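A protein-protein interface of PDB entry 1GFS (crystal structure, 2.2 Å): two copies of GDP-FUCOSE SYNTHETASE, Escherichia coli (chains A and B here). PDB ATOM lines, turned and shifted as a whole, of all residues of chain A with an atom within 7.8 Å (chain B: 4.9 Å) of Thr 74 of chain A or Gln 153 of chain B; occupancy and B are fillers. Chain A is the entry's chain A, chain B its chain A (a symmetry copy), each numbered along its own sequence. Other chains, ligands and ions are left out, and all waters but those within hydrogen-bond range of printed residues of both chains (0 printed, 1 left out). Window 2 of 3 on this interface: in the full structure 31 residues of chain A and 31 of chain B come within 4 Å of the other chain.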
ATOM      1  N   GLY A  68      -6.056  10.530   0.409  1.00  0.00           N
ATOM      2  CA  GLY A  68      -4.876  10.941   1.135  1.00  0.00           C
ATOM      3  C   GLY A  68      -5.184  11.812   2.335  1.00  0.00           C
ATOM      4  O   GLY A  68      -6.338  11.992   2.730  1.00  0.00           O
ATOM      5  N   ILE A  69      -4.113  12.357   2.897  1.00  0.00           N
ATOM      6  CA  ILE A  69      -4.127  13.230   4.061  1.00  0.00           C
ATOM      7  C   ILE A  69      -5.086  14.408   3.916  1.00  0.00           C
ATOM      8  O   ILE A  69      -5.878  14.680   4.815  1.00  0.00           O
ATOM      9  CB  ILE A  69      -2.681  13.694   4.349  1.00  0.00           C
ATOM     10  CG1 ILE A  69      -1.911  12.533   4.971  1.00  0.00           C
ATOM     11  CG2 ILE A  69      -2.643  14.897   5.259  1.00  0.00           C
ATOM     12  CD1 ILE A  69      -0.429  12.773   5.075  1.00  0.00           C
ATOM     13  N   VAL A  70      -5.034  15.082   2.771  1.00  0.00           N
ATOM     14  CA  VAL A  70      -5.910  16.220   2.517  1.00  0.00           C
ATOM     15  C   VAL A  70      -7.378  15.779   2.453  1.00  0.00           C
ATOM     16  O   VAL A  70      -8.221  16.335   3.159  1.00  0.00           O
ATOM     17  CB  VAL A  70      -5.502  17.016   1.219  1.00  0.00           C
ATOM     18  CG1 VAL A  70      -6.523  18.117   0.912  1.00  0.00           C
ATOM     19  CG2 VAL A  70      -4.126  17.658   1.406  1.00  0.00           C
ATOM     20  N   ALA A  71      -7.666  14.740   1.674  1.00  0.00           N
ATOM     21  CA  ALA A  71      -9.039  14.260   1.539  1.00  0.00           C
ATOM     22  C   ALA A  71      -9.667  13.817   2.864  1.00  0.00           C
ATOM     23  O   ALA A  71     -10.797  14.197   3.167  1.00  0.00           O
ATOM     24  CB  ALA A  71      -9.114  13.138   0.502  1.00  0.00           C
ATOM     25  N   ASN A  72      -8.933  13.043   3.660  1.00  0.00           N
ATOM     26  CA  ASN A  72      -9.450  12.569   4.945  1.00  0.00           C
ATOM     27  C   ASN A  72      -9.756  13.670   5.952  1.00  0.00           C
ATOM     28  O   ASN A  72     -10.635  13.502   6.796  1.00  0.00           O
ATOM     29  CB  ASN A  72      -8.504  11.553   5.582  1.00  0.00           C
ATOM     30  CG  ASN A  72      -8.704  10.153   5.038  1.00  0.00           C
ATOM     31  OD1 ASN A  72      -8.014   9.735   4.104  1.00  0.00           O
ATOM     32  ND2 ASN A  72      -9.659   9.425   5.612  1.00  0.00           N
ATOM     33  N   ASN A  73      -9.005  14.771   5.892  1.00  0.00           N
ATOM     34  CA  ASN A  73      -9.226  15.897   6.797  1.00  0.00           C
ATOM     35  C   ASN A  73     -10.221  16.894   6.223  1.00  0.00           C
ATOM     36  O   ASN A  73     -10.804  17.681   6.960  1.00  0.00           O
ATOM     37  CB  ASN A  73      -7.916  16.635   7.088  1.00  0.00           C
ATOM     38  CG  ASN A  73      -7.083  15.965   8.160  1.00  0.00           C
ATOM     39  OD1 ASN A  73      -7.526  15.796   9.301  1.00  0.00           O
ATOM     40  ND2 ASN A  73      -5.856  15.603   7.808  1.00  0.00           N
ATOM     41  N   THR A  74     -10.386  16.884   4.905  1.00  0.00           N
ATOM     42  CA  THR A  74     -11.295  17.802   4.243  1.00  0.00           C
ATOM     43  C   THR A  74     -12.726  17.274   4.146  1.00  0.00           C
ATOM     44  O   THR A  74     -13.682  18.032   4.315  1.00  0.00           O
ATOM     45  CB  THR A  74     -10.758  18.188   2.855  1.00  0.00           C
ATOM     46  OG1 THR A  74      -9.448  18.744   3.013  1.00  0.00           O
ATOM     47  CG2 THR A  74     -11.666  19.230   2.182  1.00  0.00           C
ATOM     48  N   TYR A  75     -12.879  15.971   3.916  1.00  0.00           N
ATOM     49  CA  TYR A  75     -14.216  15.385   3.819  1.00  0.00           C
ATOM     50  C   TYR A  75     -14.414  14.274   4.848  1.00  0.00           C
ATOM     51  O   TYR A  75     -14.789  13.171   4.486  1.00  0.00           O
ATOM     52  CB  TYR A  75     -14.434  14.798   2.426  1.00  0.00           C
ATOM     53  CG  TYR A  75     -13.986  15.688   1.295  1.00  0.00           C
ATOM     54  CD1 TYR A  75     -14.811  16.708   0.816  1.00  0.00           C
ATOM     55  CD2 TYR A  75     -12.730  15.517   0.708  1.00  0.00           C
ATOM     56  CE1 TYR A  75     -14.397  17.540  -0.226  1.00  0.00           C
ATOM     57  CE2 TYR A  75     -12.303  16.342  -0.329  1.00  0.00           C
ATOM     58  CZ  TYR A  75     -13.141  17.352  -0.791  1.00  0.00           C
ATOM     59  OH  TYR A  75     -12.721  18.178  -1.808  1.00  0.00           O
ATOM     60  N   PRO A  76     -14.202  14.556   6.145  1.00  0.00           N
ATOM     61  CA  PRO A  76     -14.381  13.496   7.144  1.00  0.00           C
ATOM     62  C   PRO A  76     -15.756  12.803   7.159  1.00  0.00           C
ATOM     63  O   PRO A  76     -15.825  11.574   7.262  1.00  0.00           O
ATOM     64  CB  PRO A  76     -14.046  14.205   8.463  1.00  0.00           C
ATOM     65  CG  PRO A  76     -14.372  15.646   8.181  1.00  0.00           C
ATOM     66  CD  PRO A  76     -13.828  15.828   6.788  1.00  0.00           C
ATOM     67  N   ALA A  77     -16.840  13.570   7.033  1.00  0.00           N
ATOM     68  CA  ALA A  77     -18.190  13.003   7.018  1.00  0.00           C
ATOM     69  C   ALA A  77     -18.405  12.013   5.868  1.00  0.00           C
ATOM     70  O   ALA A  77     -18.990  10.952   6.059  1.00  0.00           O
ATOM     71  CB  ALA A  77     -19.208  14.098   6.946  1.00  0.00           C
ATOM     72  N   ASP A  78     -17.927  12.355   4.673  1.00  0.00           N
ATOM     73  CA  ASP A  78     -18.077  11.480   3.510  1.00  0.00           C
ATOM     74  C   ASP A  78     -17.325  10.173   3.708  1.00  0.00           C
ATOM     75  O   ASP A  78     -17.801   9.114   3.312  1.00  0.00           O
ATOM     76  CB  ASP A  78     -17.559  12.155   2.231  1.00  0.00           C
ATOM     77  CG  ASP A  78     -18.310  13.440   1.877  1.00  0.00           C
ATOM     78  OD1 ASP A  78     -19.331  13.794   2.513  1.00  0.00           O
ATOM     79  OD2 ASP A  78     -17.855  14.115   0.942  1.00  0.00           O
ATOM     80  N   PHE A  79     -16.154  10.249   4.333  1.00  0.00           N
ATOM     81  CA  PHE A  79     -15.336   9.064   4.568  1.00  0.00           C
ATOM     82  C   PHE A  79     -15.920   8.090   5.574  1.00  0.00           C
ATOM     83  O   PHE A  79     -15.864   6.879   5.356  1.00  0.00           O
ATOM     84  CB  PHE A  79     -13.917   9.443   4.970  1.00  0.00           C
ATOM     85  CG  PHE A  79     -13.033   9.773   3.804  1.00  0.00           C
ATOM     86  CD1 PHE A  79     -13.053  11.037   3.230  1.00  0.00           C
ATOM     87  CD2 PHE A  79     -12.169   8.817   3.283  1.00  0.00           C
ATOM     88  CE1 PHE A  79     -12.225  11.344   2.154  1.00  0.00           C
ATOM     89  CE2 PHE A  79     -11.335   9.119   2.204  1.00  0.00           C
ATOM     90  CZ  PHE A  79     -11.363  10.383   1.641  1.00  0.00           C
ATOM     91  N   ILE A  80     -16.467   8.601   6.676  1.00  0.00           N
ATOM     92  CA  ILE A  80     -17.059   7.708   7.665  1.00  0.00           C
ATOM     93  C   ILE A  80     -18.424   7.193   7.202  1.00  0.00           C
ATOM     94  O   ILE A  80     -18.669   5.990   7.206  1.00  0.00           O
ATOM     95  CB  ILE A  80     -17.132   8.332   9.112  1.00  0.00           C
ATOM     96  CG1 ILE A  80     -17.675   7.287  10.089  1.00  0.00           C
ATOM     97  CG2 ILE A  80     -17.988   9.603   9.152  1.00  0.00           C
ATOM     98  CD1 ILE A  80     -17.477   7.634  11.549  1.00  0.00           C
ATOM     99  N   GLN A  82     -19.894   7.046   4.020  1.00  0.00           N
ATOM    100  CA  GLN A  82     -19.889   6.176   2.861  1.00  0.00           C
ATOM    101  C   GLN A  82     -19.310   4.807   3.118  1.00  0.00           C
ATOM    102  O   GLN A  82     -19.803   3.824   2.587  1.00  0.00           O
ATOM    103  CB  GLN A  82     -19.184   6.844   1.687  1.00  0.00           C
ATOM    104  CG  GLN A  82     -20.017   7.915   1.041  1.00  0.00           C
ATOM    105  CD  GLN A  82     -19.259   8.678  -0.012  1.00  0.00           C
ATOM    106  OE1 GLN A  82     -19.470   9.873  -0.190  1.00  0.00           O
ATOM    107  NE2 GLN A  82     -18.357   8.002  -0.708  1.00  0.00           N
ATOM    108  N   THR A 132      -5.926  12.322  11.613  1.00  0.00           N
ATOM    109  CA  THR A 132      -6.162  12.401  10.179  1.00  0.00           C
ATOM    110  C   THR A 132      -7.041  11.276   9.662  1.00  0.00           C
ATOM    111  O   THR A 132      -7.961  11.516   8.879  1.00  0.00           O
ATOM    112  CB  THR A 132      -4.845  12.387   9.393  1.00  0.00           C
ATOM    113  OG1 THR A 132      -4.117  13.587   9.675  1.00  0.00           O
ATOM    114  CG2 THR A 132      -5.111  12.293   7.883  1.00  0.00           C
ATOM    115  N   SER B 149     -17.736  14.357  12.581  1.00  0.00           N
ATOM    116  CA  SER B 149     -17.364  14.476  11.173  1.00  0.00           C
ATOM    117  C   SER B 149     -18.267  15.433  10.397  1.00  0.00           C
ATOM    118  O   SER B 149     -17.788  16.121   9.503  1.00  0.00           O
ATOM    119  CB  SER B 149     -17.328  13.095  10.507  1.00  0.00           C
ATOM    120  OG  SER B 149     -16.327  12.283  11.108  1.00  0.00           O
ATOM    121  N   TYR B 150     -19.564  15.459  10.726  1.00  0.00           N
ATOM    122  CA  TYR B 150     -20.512  16.366  10.072  1.00  0.00           C
ATOM    123  C   TYR B 150     -20.314  17.769  10.617  1.00  0.00           C
ATOM    124  O   TYR B 150     -20.523  18.739   9.900  1.00  0.00           O
ATOM    125  CB  TYR B 150     -21.971  15.916  10.244  1.00  0.00           C
ATOM    126  CG  TYR B 150     -22.391  14.853   9.245  1.00  0.00           C
ATOM    127  CD1 TYR B 150     -22.025  13.512   9.422  1.00  0.00           C
ATOM    128  CD2 TYR B 150     -23.078  15.194   8.081  1.00  0.00           C
ATOM    129  CE1 TYR B 150     -22.327  12.541   8.460  1.00  0.00           C
ATOM    130  CE2 TYR B 150     -23.392  14.221   7.108  1.00  0.00           C
ATOM    131  CZ  TYR B 150     -23.008  12.907   7.307  1.00  0.00           C
ATOM    132  OH  TYR B 150     -23.288  11.959   6.352  1.00  0.00           O
ATOM    133  N   ASN B 151     -19.911  17.869  11.882  1.00  0.00           N
ATOM    134  CA  ASN B 151     -19.640  19.167  12.494  1.00  0.00           C
ATOM    135  C   ASN B 151     -18.408  19.788  11.833  1.00  0.00           C
ATOM    136  O   ASN B 151     -18.398  20.970  11.513  1.00  0.00           O
ATOM    137  CB  ASN B 151     -19.362  19.036  13.990  1.00  0.00           C
ATOM    138  CG  ASN B 151     -20.587  18.655  14.795  1.00  0.00           C
ATOM    139  OD1 ASN B 151     -20.463  18.304  15.961  1.00  0.00           O
ATOM    140  ND2 ASN B 151     -21.758  18.710  14.191  1.00  0.00           N
ATOM    141  N   ARG B 152     -17.357  18.986  11.677  1.00  0.00           N
ATOM    142  CA  ARG B 152     -16.111  19.424  11.050  1.00  0.00           C
ATOM    143  C   ARG B 152     -16.284  19.775   9.565  1.00  0.00           C
ATOM    144  O   ARG B 152     -15.993  20.897   9.155  1.00  0.00           O
ATOM    145  CB  ARG B 152     -15.029  18.351  11.221  1.00  0.00           C
ATOM    146  CG  ARG B 152     -14.504  18.243  12.647  1.00  0.00           C
ATOM    147  CD  ARG B 152     -13.541  17.081  12.817  1.00  0.00           C
ATOM    148  NE  ARG B 152     -12.287  17.296  12.108  1.00  0.00           N
ATOM    149  CZ  ARG B 152     -11.634  16.361  11.422  1.00  0.00           C
ATOM    150  NH1 ARG B 152     -12.112  15.125  11.338  1.00  0.00           N
ATOM    151  NH2 ARG B 152     -10.476  16.652  10.840  1.00  0.00           N
ATOM    152  N   GLN B 153     -16.816  18.841   8.779  1.00  0.00           N
ATOM    153  CA  GLN B 153     -17.001  19.059   7.349  1.00  0.00           C
ATOM    154  C   GLN B 153     -18.075  20.061   6.965  1.00  0.00           C
ATOM    155  O   GLN B 153     -17.815  20.955   6.185  1.00  0.00           O
ATOM    156  CB  GLN B 153     -17.281  17.742   6.609  1.00  0.00           C
ATOM    157  CG  GLN B 153     -17.350  17.906   5.078  1.00  0.00           C
ATOM    158  CD  GLN B 153     -17.478  16.589   4.301  1.00  0.00           C
ATOM    159  OE1 GLN B 153     -17.930  16.573   3.157  1.00  0.00           O
ATOM    160  NE2 GLN B 153     -17.072  15.498   4.908  1.00  0.00           N
ATOM    161  N   TYR B 154     -19.271  19.926   7.524  1.00  0.00           N
ATOM    162  CA  TYR B 154     -20.380  20.793   7.139  1.00  0.00           C
ATOM    163  C   TYR B 154     -20.752  21.928   8.074  1.00  0.00           C
ATOM    164  O   TYR B 154     -21.665  22.697   7.780  1.00  0.00           O
ATOM    165  CB  TYR B 154     -21.617  19.933   6.821  1.00  0.00           C
ATOM    166  CG  TYR B 154     -21.402  18.930   5.686  1.00  0.00           C
ATOM    167  CD1 TYR B 154     -21.294  19.360   4.350  1.00  0.00           C
ATOM    168  CD2 TYR B 154     -21.310  17.555   5.938  1.00  0.00           C
ATOM    169  CE1 TYR B 154     -21.097  18.454   3.305  1.00  0.00           C
ATOM    170  CE2 TYR B 154     -21.117  16.637   4.889  1.00  0.00           C
ATOM    171  CZ  TYR B 154     -21.008  17.098   3.577  1.00  0.00           C
ATOM    172  OH  TYR B 154     -20.780  16.212   2.539  1.00  0.00           O
ATOM    173  N   GLY B 155     -20.033  22.061   9.176  1.00  0.00           N
ATOM    174  CA  GLY B 155     -20.338  23.119  10.115  1.00  0.00           C
ATOM    175  C   GLY B 155     -21.643  22.874  10.840  1.00  0.00           C
ATOM    176  O   GLY B 155     -22.351  23.813  11.178  1.00  0.00           O
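OE1 of Gln 153 of chain B sits close to OD1 of Asp 78 of chain A (3.2 Å). The backbone NH of Ala 77 of chain A sits close to the side-chain amide nitrogen of Gln 153 of chain B, at 2.9 Å. The backbone carbonyl oxygen (O) of Tyr 75 of chain A lies close to the side-chain amide nitrogen (NE2) of Gln 153 of chain B, 3.3 Å away. The guanidinium group (NH2) of Arg 152 of chain B lies within hydrogen-bond range of the side-chain amide oxygen (OD1) of Asn 73 of chain A, at 3.4 Å. NE2 of Gln 153 of chain B sits close to N of Pro 76 of chain A, 3.3 Å away. OD1 of Asp 78 of chain A is in hydrogen-bond range of OH of Tyr 154 of chain B.
The side-chain amide nitrogen of Asn 73 of chain A lies within hydrogen-bond range of the backbone carbonyl oxygen of Ile 69 of chain A. The side-chain hydroxyl (OG1) of Thr 74 of chain A is in hydrogen-bond range of the backbone carbonyl oxygen (O) of Val 70 of chain A (2.7 Å). The side-chain amide oxygen (OE1) of Gln 153 of chain B is in hydrogen-bond range of the side-chain hydroxyl (OH) of Tyr 154 of chain B. The backbone carbonyl oxygen of Tyr 150 of chain B is in hydrogen-bond range of the backbone NH of Gly 155 of chain B, at 3.4 Å. The side-chain amide nitrogen (ND2) of Asn 73 of chain A is in hydrogen-bond range of the side-chain hydroxyl (OG1) of Thr 132 of chain A (3.3 Å).
CG of Gln 153 of chain B touches O of Thr 74 of chain A, 3.7 Å away. O of Ser 149 of chain B touches CG of Pro 76 of chain A (3.7 Å). NH1 of Arg 152 of chain B touches CB of Pro 76 of chain A, 3.6 Å away. N of Ala 77 of chain A touches CB of Ser 149 of chain B, 3.5 Å away. CD1 of Tyr 150 of chain B touches CB of Ala 77 of chain A (3.8 Å). CB of Ala 77 of chain A touches CE2 of Tyr 154 of chain B (3.8 Å). Ile 80 of chain A touches Ser 149 of chain B.
Of the printed residues of chain B, Thr 74 of chain A touches Gln 153. Printed residues of chain A within 4 Å of Gln 153 of chain B: Thr 74 (3.7 Å), Tyr 75 (2.9 Å), Pro 76 (3.3 Å), Ala 77 (2.9 Å) and Asp 78 (3.2 Å). Of the printed residues of chain B, Ile 80 of chain A touches Ser 149 (3.7 Å). Of the printed residues of chain B, Tyr 75 of chain A touches Gln 153. Of the printed residues of chain B, Asp 78 of chain A touches Gln 153 and Tyr 154. The nearest residue of chain A that does not touch Gln 153 of chain B is Phe 79 of chain A (5.4 Å). The nearest printed residue of chain B that does not touch Pro 76 of chain A is Tyr 150 of chain B (5.8 Å).
Of the 15 printed residues of chain A, 7 touch a printed residue of chain B. Hydrophobic or aromatic side chains of chain A within 4 Å of the printed part of chain B: Tyr 75, Pro 76, Ala 77 and Ile 80. Printed residues of chain B that touch a printed residue of chain A: Ser 149, Tyr 150, Arg 152, Gln 153 and Tyr 154. Hydrophobic or aromatic side chains of chain B within 4 Å of the printed part of chain A: Tyr 150 and Tyr 154. Among the printed residues, no Asp or Glu carboxylate lies within 4 Å of a Lys or Arg side-chain nitrogen of the other chain.
No position is printed for both chains.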
